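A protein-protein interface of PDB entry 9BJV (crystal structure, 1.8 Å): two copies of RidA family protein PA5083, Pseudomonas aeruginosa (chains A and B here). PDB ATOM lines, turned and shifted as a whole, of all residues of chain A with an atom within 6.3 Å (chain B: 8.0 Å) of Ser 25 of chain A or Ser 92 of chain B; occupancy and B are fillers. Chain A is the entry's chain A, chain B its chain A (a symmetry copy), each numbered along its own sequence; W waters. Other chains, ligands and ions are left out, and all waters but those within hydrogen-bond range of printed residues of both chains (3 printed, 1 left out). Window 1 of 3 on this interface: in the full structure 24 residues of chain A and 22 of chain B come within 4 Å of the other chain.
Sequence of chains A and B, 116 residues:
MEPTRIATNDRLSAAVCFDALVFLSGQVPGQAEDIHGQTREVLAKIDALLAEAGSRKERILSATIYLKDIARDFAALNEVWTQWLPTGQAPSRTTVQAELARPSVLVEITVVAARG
O of Pro 91 of chain B sits at hydrogen-bond distance from N of Ser 13 of chain A (2.9 Å).
OG of Ser 25 of chain A sits at hydrogen-bond distance from N of Arg 93 of chain B, at 2.9 Å.
O of Arg 93 of chain B is in hydrogen-bond range of N of Gly 26 of chain A (3.1 Å).
N of Gly 26 of chain A lies within hydrogen-bond range of OG1 of Thr 94 of chain B (3.0 Å).
The side-chain hydroxyl of Thr 110 of chain A sits at hydrogen-bond distance from the side-chain hydroxyl of Thr 94 of chain B (2.8 Å).
The side-chain hydroxyl (OG) of Ser 13 of chain A is in hydrogen-bond range of the backbone carbonyl oxygen (O) of Ala 90 of chain B (2.7 Å).
OG1 of Thr 95 of chain B is in hydrogen-bond range of NE of Arg 93 of chain B, at 3.4 Å.
The backbone carbonyl oxygen (O) of Ser 25 of chain A lies within hydrogen-bond range of the side-chain amide nitrogen (NE2) of Gln 27 of chain A.
The backbone carbonyl oxygen (O) of Val 112 of chain B is in hydrogen-bond range of the backbone NH (N) of Leu 61 of chain B.
The backbone carbonyl oxygen (O) of Thr 94 of chain B lies within hydrogen-bond range of the backbone NH (N) of Ile 65 of chain B.
The backbone carbonyl oxygen (O) of Leu 61 of chain B is in hydrogen-bond range of the side-chain hydroxyl (OG) of Ser 92 of chain B, at 2.7 Å.
The backbone NH of Leu 24 of chain A is in hydrogen-bond range of the backbone carbonyl oxygen of Val 111 of chain A, 3.0 Å away.
Ala 90 of chain B touches Leu 12 of chain A.
Pro 91 of chain B touches Leu 12 of chain A (O to CA, 3.3 Å).
Arg 93 of chain B touches Leu 12 of chain A.
Ser 13 of chain A touches Ser 92 of chain B.
Leu 61 of chain B touches Val 16 of chain A.
C of Pro 91 of chain B touches CG2 of Val 16 of chain A (3.9 Å).
Val 16 of chain A touches Ser 92 of chain B.
Ser 92 of chain B touches Leu 24 of chain A (CB to C, 3.8 Å).
Ser 25 of chain A touches Ser 92 of chain B (OG to CA, 3.4 Å).
Thr 94 of chain B touches Glu 108 of chain A.
Of the printed residues of chain B, Phe 23 of chain A touches Leu 61 (3.8 Å) and Ser 92 (3.4 Å).
Of the printed residues of chain B, Leu 24 of chain A touches Ser 92 (3.8 Å).
Ser 25 of chain A touches two residues of chain B.
Of chain B, only Arg 93 and Thr 94 come within 4 Å of Gly 26 of chain A.
Of the printed residues of chain A, Ser 92 of chain B touches Ser 13, Val 16, Phe 23, Leu 24 and Ser 25.
The nearest residue of chain B that does not touch Ser 25 of chain A is Thr 94 of chain B (4.1 Å).
The nearest residue of chain A that does not touch Ser 92 of chain B is Leu 12 of chain A (4.9 Å).
The nearest printed residue of chain A that does not touch Ala 90 of chain B is Val 16 of chain A (4.2 Å).
Printed residues of chain A that touch a printed residue of chain B: Leu 12, Ser 13, Val 16, Phe 23, Leu 24, Ser 25, Gly 26, Glu 108 and Thr 110.
Of the 17 printed residues of chain B, 6 touch a printed residue of chain A.
Printed residues of chain B that touch a printed residue of chain A: Leu 61, Ala 90, Pro 91, Ser 92, Arg 93 and Thr 94.
Among the printed residues, no Asp or Glu carboxylate lies within 4 Å of a Lys or Arg side-chain nitrogen of the other chain.
Positions printed for both chains: 110 and 111.
Water W2 bridges the side-chain carboxylate of Glu 108 of chain A (2.5 Å) and the backbone NH of Thr 95 of chain B (2.9 Å).
Water W3 bridges the backbone carbonyl oxygen (O) of Thr 95 of chain B (2.7 Å) and the side-chain carboxylate (OE1) of Glu 108 of chain A (2.8 Å).
Water W1 bridges O of Leu 24 of chain A (2.7 Å) and OG of Ser 92 of chain B (2.7 Å).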
ATOM      1  N   LEU A  12      30.623 -29.413 -23.014  1.00  0.00           N
ATOM      2  CA  LEU A  12      29.188 -29.627 -23.138  1.00  0.00           C
ATOM      3  C   LEU A  12      28.789 -30.883 -22.381  1.00  0.00           C
ATOM      4  O   LEU A  12      29.625 -31.729 -22.047  1.00  0.00           O
ATOM      5  CB  LEU A  12      28.765 -29.747 -24.610  1.00  0.00           C
ATOM      6  CG  LEU A  12      29.409 -30.865 -25.446  1.00  0.00           C
ATOM      7  CD1 LEU A  12      28.668 -32.211 -25.322  1.00  0.00           C
ATOM      8  CD2 LEU A  12      29.534 -30.443 -26.906  1.00  0.00           C
ATOM      9  N   SER A  13      27.484 -31.001 -22.137  1.00  0.00           N
ATOM     10  CA  SER A  13      26.866 -32.255 -21.749  1.00  0.00           C
ATOM     11  C   SER A  13      26.030 -32.761 -22.919  1.00  0.00           C
ATOM     12  O   SER A  13      25.312 -31.985 -23.561  1.00  0.00           O
ATOM     13  CB  SER A  13      25.972 -32.101 -20.511  1.00  0.00           C
ATOM     14  OG  SER A  13      26.703 -31.638 -19.385  1.00  0.00           O
ATOM     15  N   ALA A  14      26.118 -34.066 -23.184  1.00  0.00           N
ATOM     16  CA  ALA A  14      25.342 -34.642 -24.279  1.00  0.00           C
ATOM     17  C   ALA A  14      23.853 -34.400 -24.090  1.00  0.00           C
ATOM     18  O   ALA A  14      23.123 -34.239 -25.075  1.00  0.00           O
ATOM     19  CB  ALA A  14      25.617 -36.144 -24.399  1.00  0.00           C
ATOM     20  N   ALA A  15      23.382 -34.388 -22.839  1.00  0.00           N
ATOM     21  CA  ALA A  15      21.980 -34.127 -22.538  1.00  0.00           C
ATOM     22  C   ALA A  15      21.873 -33.379 -21.219  1.00  0.00           C
ATOM     23  O   ALA A  15      22.636 -33.638 -20.282  1.00  0.00           O
ATOM     24  CB  ALA A  15      21.160 -35.414 -22.444  1.00  0.00           C
ATOM     25  N   VAL A  16      20.910 -32.465 -21.154  1.00  0.00           N
ATOM     26  CA  VAL A  16      20.558 -31.768 -19.926  1.00  0.00           C
ATOM     27  C   VAL A  16      19.056 -31.888 -19.752  1.00  0.00           C
ATOM     28  O   VAL A  16      18.299 -31.564 -20.671  1.00  0.00           O
ATOM     29  CB  VAL A  16      20.984 -30.289 -19.958  1.00  0.00           C
ATOM     30  CG1 VAL A  16      20.466 -29.570 -18.717  1.00  0.00           C
ATOM     31  CG2 VAL A  16      22.505 -30.172 -20.062  1.00  0.00           C
ATOM     32  N   PHE A  23      17.151 -31.560 -23.290  1.00  0.00           N
ATOM     33  CA  PHE A  23      17.893 -30.773 -24.274  1.00  0.00           C
ATOM     34  C   PHE A  23      19.143 -31.544 -24.681  1.00  0.00           C
ATOM     35  O   PHE A  23      20.020 -31.775 -23.845  1.00  0.00           O
ATOM     36  CB  PHE A  23      18.300 -29.412 -23.704  1.00  0.00           C
ATOM     37  CG  PHE A  23      17.135 -28.571 -23.256  1.00  0.00           C
ATOM     38  CD1 PHE A  23      16.526 -28.801 -22.028  1.00  0.00           C
ATOM     39  CD2 PHE A  23      16.659 -27.548 -24.061  1.00  0.00           C
ATOM     40  CE1 PHE A  23      15.442 -28.027 -21.609  1.00  0.00           C
ATOM     41  CE2 PHE A  23      15.576 -26.770 -23.654  1.00  0.00           C
ATOM     42  CZ  PHE A  23      14.971 -27.010 -22.420  1.00  0.00           C
ATOM     43  N   LEU A  24      19.238 -31.918 -25.953  1.00  0.00           N
ATOM     44  CA  LEU A  24      20.387 -32.670 -26.446  1.00  0.00           C
ATOM     45  C   LEU A  24      21.377 -31.759 -27.159  1.00  0.00           C
ATOM     46  O   LEU A  24      20.984 -30.882 -27.931  1.00  0.00           O
ATOM     47  CB  LEU A  24      19.943 -33.773 -27.410  1.00  0.00           C
ATOM     48  CG  LEU A  24      18.982 -34.819 -26.852  1.00  0.00           C
ATOM     49  CD1 LEU A  24      18.816 -35.966 -27.852  1.00  0.00           C
ATOM     50  CD2 LEU A  24      19.508 -35.332 -25.523  1.00  0.00           C
ATOM     51  N   SER A  25      22.667 -31.982 -26.913  1.00  0.00           N
ATOM     52  CA  SER A  25      23.677 -31.364 -27.760  1.00  0.00           C
ATOM     53  C   SER A  25      23.485 -31.804 -29.208  1.00  0.00           C
ATOM     54  O   SER A  25      22.981 -32.898 -29.490  1.00  0.00           O
ATOM     55  CB  SER A  25      25.083 -31.735 -27.281  1.00  0.00           C
ATOM     56  OG  SER A  25      25.397 -31.089 -26.048  1.00  0.00           O
ATOM     57  N   GLY A  26      23.870 -30.933 -30.136  1.00  0.00           N
ATOM     58  CA  GLY A  26      23.871 -31.329 -31.533  1.00  0.00           C
ATOM     59  C   GLY A  26      24.694 -32.593 -31.710  1.00  0.00           C
ATOM     60  O   GLY A  26      25.814 -32.683 -31.190  1.00  0.00           O
ATOM     61  N   GLN A  27      24.157 -33.577 -32.429  1.00  0.00           N
ATOM     62  CA  GLN A  27      24.836 -34.855 -32.610  1.00  0.00           C
ATOM     63  C   GLN A  27      25.439 -34.921 -34.004  1.00  0.00           C
ATOM     64  O   GLN A  27      24.802 -34.517 -34.980  1.00  0.00           O
ATOM     65  CB  GLN A  27      23.872 -36.020 -32.382  1.00  0.00           C
ATOM     66  CG  GLN A  27      23.392 -36.093 -30.954  1.00  0.00           C
ATOM     67  CD  GLN A  27      24.558 -36.211 -29.991  1.00  0.00           C
ATOM     68  OE1 GLN A  27      25.371 -37.136 -30.102  1.00  0.00           O
ATOM     69  NE2 GLN A  27      24.671 -35.261 -29.064  1.00  0.00           N
ATOM     70  N   ILE A  46      21.243 -39.858 -31.338  1.00  0.00           N
ATOM     71  CA  ILE A  46      20.102 -39.182 -30.718  1.00  0.00           C
ATOM     72  C   ILE A  46      19.195 -40.191 -30.025  1.00  0.00           C
ATOM     73  O   ILE A  46      18.729 -39.981 -28.900  1.00  0.00           O
ATOM     74  CB  ILE A  46      19.337 -38.383 -31.785  1.00  0.00           C
ATOM     75  CG1 ILE A  46      20.195 -37.205 -32.253  1.00  0.00           C
ATOM     76  CG2 ILE A  46      17.956 -37.951 -31.273  1.00  0.00           C
ATOM     77  CD1 ILE A  46      19.506 -36.339 -33.323  1.00  0.00           C
ATOM     78  N   LEU A  49      20.696 -41.162 -26.693  1.00  0.00           N
ATOM     79  CA  LEU A  49      20.632 -40.096 -25.696  1.00  0.00           C
ATOM     80  C   LEU A  49      19.217 -39.926 -25.165  1.00  0.00           C
ATOM     81  O   LEU A  49      19.023 -39.718 -23.962  1.00  0.00           O
ATOM     82  CB  LEU A  49      21.146 -38.783 -26.290  1.00  0.00           C
ATOM     83  CG  LEU A  49      22.650 -38.742 -26.524  1.00  0.00           C
ATOM     84  CD1 LEU A  49      23.024 -37.431 -27.209  1.00  0.00           C
ATOM     85  CD2 LEU A  49      23.408 -38.911 -25.215  1.00  0.00           C
ATOM     86  N   GLU A 108      24.285 -32.406 -38.928  1.00  0.00           N
ATOM     87  CA  GLU A 108      24.265 -32.343 -37.472  1.00  0.00           C
ATOM     88  C   GLU A 108      22.844 -32.011 -37.048  1.00  0.00           C
ATOM     89  O   GLU A 108      22.188 -31.190 -37.692  1.00  0.00           O
ATOM     90  CB  GLU A 108      25.249 -31.289 -36.916  1.00  0.00           C
ATOM     91  CG  GLU A 108      25.172 -31.145 -35.362  1.00  0.00           C
ATOM     92  CD  GLU A 108      26.341 -30.382 -34.746  1.00  0.00           C
ATOM     93  OE1 GLU A 108      27.332 -30.127 -35.468  1.00  0.00           O
ATOM     94  OE2 GLU A 108      26.276 -30.034 -33.529  1.00  0.00           O
ATOM     95  N   ILE A 109      22.346 -32.649 -35.987  1.00  0.00           N
ATOM     96  CA  ILE A 109      20.944 -32.483 -35.606  1.00  0.00           C
ATOM     97  C   ILE A 109      20.844 -32.205 -34.110  1.00  0.00           C
ATOM     98  O   ILE A 109      21.444 -32.921 -33.297  1.00  0.00           O
ATOM     99  CB  ILE A 109      20.101 -33.716 -35.994  1.00  0.00           C
ATOM    100  CG1 ILE A 109      20.179 -33.972 -37.507  1.00  0.00           C
ATOM    101  CG2 ILE A 109      18.646 -33.534 -35.578  1.00  0.00           C
ATOM    102  CD1 ILE A 109      19.379 -35.201 -37.965  1.00  0.00           C
ATOM    103  N   THR A 110      20.062 -31.182 -33.752  1.00  0.00           N
ATOM    104  CA  THR A 110      19.888 -30.736 -32.371  1.00  0.00           C
ATOM    105  C   THR A 110      18.437 -30.933 -31.957  1.00  0.00           C
ATOM    106  O   THR A 110      17.531 -30.331 -32.551  1.00  0.00           O
ATOM    107  CB  THR A 110      20.274 -29.265 -32.228  1.00  0.00           C
ATOM    108  OG1 THR A 110      21.629 -29.101 -32.643  1.00  0.00           O
ATOM    109  CG2 THR A 110      20.086 -28.782 -30.780  1.00  0.00           C
ATOM    110  N   VAL A 111      18.215 -31.748 -30.927  1.00  0.00           N
ATOM    111  CA  VAL A 111      16.873 -32.171 -30.541  1.00  0.00           C
ATOM    112  C   VAL A 111      16.531 -31.662 -29.144  1.00  0.00           C
ATOM    113  O   VAL A 111      17.374 -31.675 -28.242  1.00  0.00           O
ATOM    114  CB  VAL A 111      16.749 -33.710 -30.602  1.00  0.00           C
ATOM    115  CG1 VAL A 111      15.652 -34.226 -29.636  1.00  0.00           C
ATOM    116  CG2 VAL A 111      16.488 -34.167 -32.041  1.00  0.00           C
ATOM    117  N   ILE B  60      22.174 -23.116 -17.122  1.00  0.00           N
ATOM    118  CA  ILE B  60      21.992 -23.104 -18.570  1.00  0.00           C
ATOM    119  C   ILE B  60      21.574 -24.492 -19.040  1.00  0.00           C
ATOM    120  O   ILE B  60      22.143 -25.513 -18.626  1.00  0.00           O
ATOM    121  CB  ILE B  60      23.283 -22.634 -19.261  1.00  0.00           C
ATOM    122  CG1 ILE B  60      23.671 -21.232 -18.771  1.00  0.00           C
ATOM    123  CG2 ILE B  60      23.112 -22.619 -20.787  1.00  0.00           C
ATOM    124  CD1 ILE B  60      25.092 -20.798 -19.171  1.00  0.00           C
ATOM    125  N   LEU B  61      20.573 -24.536 -19.913  1.00  0.00           N
ATOM    126  CA  LEU B  61      20.083 -25.787 -20.479  1.00  0.00           C
ATOM    127  C   LEU B  61      20.636 -26.050 -21.878  1.00  0.00           C
ATOM    128  O   LEU B  61      21.000 -27.193 -22.193  1.00  0.00           O
ATOM    129  CB  LEU B  61      18.547 -25.777 -20.522  1.00  0.00           C
ATOM    130  CG  LEU B  61      17.876 -25.467 -19.173  1.00  0.00           C
ATOM    131  CD1 LEU B  61      16.382 -25.180 -19.345  1.00  0.00           C
ATOM    132  CD2 LEU B  61      18.108 -26.613 -18.191  1.00  0.00           C
ATOM    133  N   SER B  62      20.729 -25.015 -22.713  1.00  0.00           N
ATOM    134  CA  SER B  62      21.199 -25.177 -24.082  1.00  0.00           C
ATOM    135  C   SER B  62      21.901 -23.910 -24.537  1.00  0.00           C
ATOM    136  O   SER B  62      21.555 -22.803 -24.119  1.00  0.00           O
ATOM    137  CB  SER B  62      20.041 -25.488 -25.043  1.00  0.00           C
ATOM    138  OG  SER B  62      19.114 -24.416 -25.060  1.00  0.00           O
ATOM    139  N   ALA B  63      22.863 -24.079 -25.435  1.00  0.00           N
ATOM    140  CA  ALA B  63      23.510 -22.950 -26.088  1.00  0.00           C
ATOM    141  C   ALA B  63      23.759 -23.312 -27.540  1.00  0.00           C
ATOM    142  O   ALA B  63      24.364 -24.345 -27.811  1.00  0.00           O
ATOM    143  CB  ALA B  63      24.847 -22.604 -25.410  1.00  0.00           C
ATOM    144  N   THR B  64      23.278 -22.490 -28.467  1.00  0.00           N
ATOM    145  CA  THR B  64      23.740 -22.552 -29.844  1.00  0.00           C
ATOM    146  C   THR B  64      24.817 -21.494 -30.012  1.00  0.00           C
ATOM    147  O   THR B  64      24.590 -20.319 -29.710  1.00  0.00           O
ATOM    148  CB  THR B  64      22.616 -22.314 -30.855  1.00  0.00           C
ATOM    149  OG1 THR B  64      21.552 -23.246 -30.609  1.00  0.00           O
ATOM    150  CG2 THR B  64      23.159 -22.538 -32.258  1.00  0.00           C
ATOM    151  N   ILE B  65      25.991 -21.923 -30.467  1.00  0.00           N
ATOM    152  CA  ILE B  65      27.135 -21.041 -30.680  1.00  0.00           C
ATOM    153  C   ILE B  65      27.323 -20.885 -32.183  1.00  0.00           C
ATOM    154  O   ILE B  65      27.600 -21.865 -32.882  1.00  0.00           O
ATOM    155  CB  ILE B  65      28.403 -21.608 -30.013  1.00  0.00           C
ATOM    156  CG1 ILE B  65      28.183 -21.743 -28.503  1.00  0.00           C
ATOM    157  CG2 ILE B  65      29.618 -20.726 -30.308  1.00  0.00           C
ATOM    158  CD1 ILE B  65      29.411 -22.276 -27.723  1.00  0.00           C
ATOM    159  N   TRP B  81      35.215 -20.417 -23.655  1.00  0.00           N
ATOM    160  CA  TRP B  81      33.994 -21.073 -23.197  1.00  0.00           C
ATOM    161  C   TRP B  81      34.257 -21.989 -22.004  1.00  0.00           C
ATOM    162  O   TRP B  81      33.562 -21.915 -20.981  1.00  0.00           O
ATOM    163  CB  TRP B  81      33.396 -21.850 -24.376  1.00  0.00           C
ATOM    164  CG  TRP B  81      32.257 -22.783 -24.094  1.00  0.00           C
ATOM    165  CD1 TRP B  81      32.320 -24.141 -24.010  1.00  0.00           C
ATOM    166  CD2 TRP B  81      30.872 -22.434 -23.933  1.00  0.00           C
ATOM    167  NE1 TRP B  81      31.070 -24.661 -23.784  1.00  0.00           N
ATOM    168  CE2 TRP B  81      30.163 -23.634 -23.731  1.00  0.00           C
ATOM    169  CE3 TRP B  81      30.168 -21.224 -23.920  1.00  0.00           C
ATOM    170  CZ2 TRP B  81      28.783 -23.662 -23.521  1.00  0.00           C
ATOM    171  CZ3 TRP B  81      28.797 -21.255 -23.708  1.00  0.00           C
ATOM    172  CH2 TRP B  81      28.121 -22.465 -23.511  1.00  0.00           C
ATOM    173  N   GLN B  89      29.543 -28.492 -15.022  1.00  0.00           N
ATOM    174  CA  GLN B  89      28.141 -28.129 -15.219  1.00  0.00           C
ATOM    175  C   GLN B  89      27.895 -27.555 -16.612  1.00  0.00           C
ATOM    176  O   GLN B  89      27.066 -26.661 -16.800  1.00  0.00           O
ATOM    177  CB  GLN B  89      27.692 -27.168 -14.119  1.00  0.00           C
ATOM    178  CG  GLN B  89      27.736 -27.860 -12.749  1.00  0.00           C
ATOM    179  CD  GLN B  89      27.407 -26.948 -11.599  1.00  0.00           C
ATOM    180  OE1 GLN B  89      26.270 -26.910 -11.130  1.00  0.00           O
ATOM    181  NE2 GLN B  89      28.406 -26.216 -11.121  1.00  0.00           N
ATOM    182  N   ALA B  90      28.570 -28.106 -17.620  1.00  0.00           N
ATOM    183  CA  ALA B  90      28.410 -27.612 -18.983  1.00  0.00           C
ATOM    184  C   ALA B  90      27.008 -27.912 -19.513  1.00  0.00           C
ATOM    185  O   ALA B  90      26.435 -28.966 -19.213  1.00  0.00           O
ATOM    186  CB  ALA B  90      29.461 -28.237 -19.904  1.00  0.00           C
ATOM    187  N   PRO B  91      26.438 -27.020 -20.327  1.00  0.00           N
ATOM    188  CA  PRO B  91      25.081 -27.239 -20.836  1.00  0.00           C
ATOM    189  C   PRO B  91      25.083 -28.068 -22.111  1.00  0.00           C
ATOM    190  O   PRO B  91      26.155 -28.414 -22.615  1.00  0.00           O
ATOM    191  CB  PRO B  91      24.592 -25.812 -21.113  1.00  0.00           C
ATOM    192  CG  PRO B  91      25.876 -25.116 -21.607  1.00  0.00           C
ATOM    193  CD  PRO B  91      27.007 -25.739 -20.784  1.00  0.00           C
ATOM    194  N   SER B  92      23.907 -28.372 -22.655  1.00  0.00           N
ATOM    195  CA  SER B  92      23.870 -28.904 -24.013  1.00  0.00           C
ATOM    196  C   SER B  92      24.317 -27.810 -24.975  1.00  0.00           C
ATOM    197  O   SER B  92      24.103 -26.620 -24.729  1.00  0.00           O
ATOM    198  CB  SER B  92      22.469 -29.415 -24.372  1.00  0.00           C
ATOM    199  OG  SER B  92      21.539 -28.364 -24.603  1.00  0.00           O
ATOM    200  N   ARG B  93      24.972 -28.214 -26.066  1.00  0.00           N
ATOM    201  CA  ARG B  93      25.627 -27.234 -26.923  1.00  0.00           C
ATOM    202  C   ARG B  93      25.577 -27.659 -28.384  1.00  0.00           C
ATOM    203  O   ARG B  93      25.678 -28.844 -28.702  1.00  0.00           O
ATOM    204  CB  ARG B  93      27.089 -27.045 -26.487  1.00  0.00           C
ATOM    205  CG  ARG B  93      27.804 -25.917 -27.185  1.00  0.00           C
ATOM    206  CD  ARG B  93      29.242 -25.779 -26.679  1.00  0.00           C
ATOM    207  NE  ARG B  93      30.196 -26.507 -27.509  1.00  0.00           N
ATOM    208  CZ  ARG B  93      31.489 -26.209 -27.580  1.00  0.00           C
ATOM    209  NH1 ARG B  93      32.007 -25.210 -26.883  1.00  0.00           N
ATOM    210  NH2 ARG B  93      32.278 -26.923 -28.375  1.00  0.00           N
ATOM    211  N   THR B  94      25.445 -26.676 -29.270  1.00  0.00           N
ATOM    212  CA  THR B  94      25.561 -26.900 -30.705  1.00  0.00           C
ATOM    213  C   THR B  94      26.382 -25.754 -31.275  1.00  0.00           C
ATOM    214  O   THR B  94      26.062 -24.595 -31.010  1.00  0.00           O
ATOM    215  CB  THR B  94      24.179 -26.944 -31.376  1.00  0.00           C
ATOM    216  OG1 THR B  94      23.403 -28.010 -30.825  1.00  0.00           O
ATOM    217  CG2 THR B  94      24.307 -27.137 -32.878  1.00  0.00           C
ATOM    218  N   THR B  95      27.431 -26.066 -32.043  1.00  0.00           N
ATOM    219  CA  THR B  95      28.327 -25.058 -32.607  1.00  0.00           C
ATOM    220  C   THR B  95      28.299 -25.177 -34.123  1.00  0.00           C
ATOM    221  O   THR B  95      28.637 -26.232 -34.670  1.00  0.00           O
ATOM    222  CB  THR B  95      29.764 -25.233 -32.094  1.00  0.00           C
ATOM    223  OG1 THR B  95      29.753 -25.368 -30.670  1.00  0.00           O
ATOM    224  CG2 THR B  95      30.610 -24.016 -32.459  1.00  0.00           C
ATOM    225  N   THR B 110      23.260 -18.128 -28.308  1.00  0.00           N
ATOM    226  CA  THR B 110      21.851 -18.100 -27.922  1.00  0.00           C
ATOM    227  C   THR B 110      21.604 -19.138 -26.837  1.00  0.00           C
ATOM    228  O   THR B 110      21.797 -20.340 -27.067  1.00  0.00           O
ATOM    229  CB  THR B 110      20.957 -18.388 -29.127  1.00  0.00           C
ATOM    230  OG1 THR B 110      21.223 -17.418 -30.139  1.00  0.00           O
ATOM    231  CG2 THR B 110      19.471 -18.370 -28.732  1.00  0.00           C
ATOM    232  N   VAL B 111      21.155 -18.684 -25.667  1.00  0.00           N
ATOM    233  CA  VAL B 111      21.051 -19.536 -24.487  1.00  0.00           C
ATOM    234  C   VAL B 111      19.595 -19.673 -24.052  1.00  0.00           C
ATOM    235  O   VAL B 111      18.831 -18.704 -24.079  1.00  0.00           O
ATOM    236  CB  VAL B 111      21.909 -18.971 -23.333  1.00  0.00           C
ATOM    237  CG1 VAL B 111      21.359 -19.414 -21.953  1.00  0.00           C
ATOM    238  CG2 VAL B 111      23.375 -19.382 -23.509  1.00  0.00           C
ATOM    239  N   VAL B 112      19.218 -20.889 -23.664  1.00  0.00           N
ATOM    240  CA  VAL B 112      18.026 -21.157 -22.870  1.00  0.00           C
ATOM    241  C   VAL B 112      18.486 -21.708 -21.524  1.00  0.00           C
ATOM    242  O   VAL B 112      19.405 -22.538 -21.468  1.00  0.00           O
ATOM    243  CB  VAL B 112      17.078 -22.143 -23.576  1.00  0.00           C
ATOM    244  CG1 VAL B 112      15.807 -22.396 -22.716  1.00  0.00           C
ATOM    245  CG2 VAL B 112      16.717 -21.621 -24.962  1.00  0.00           C
HETATM  246  O   HOH W   1      20.247 -28.434 -27.009  1.00  0.00           O
HETATM  247  O   HOH W   2      28.115 -28.834 -32.276  1.00  0.00           O
HETATM  248  O   HOH W   3      29.640 -28.599 -35.380  1.00  0.00           O
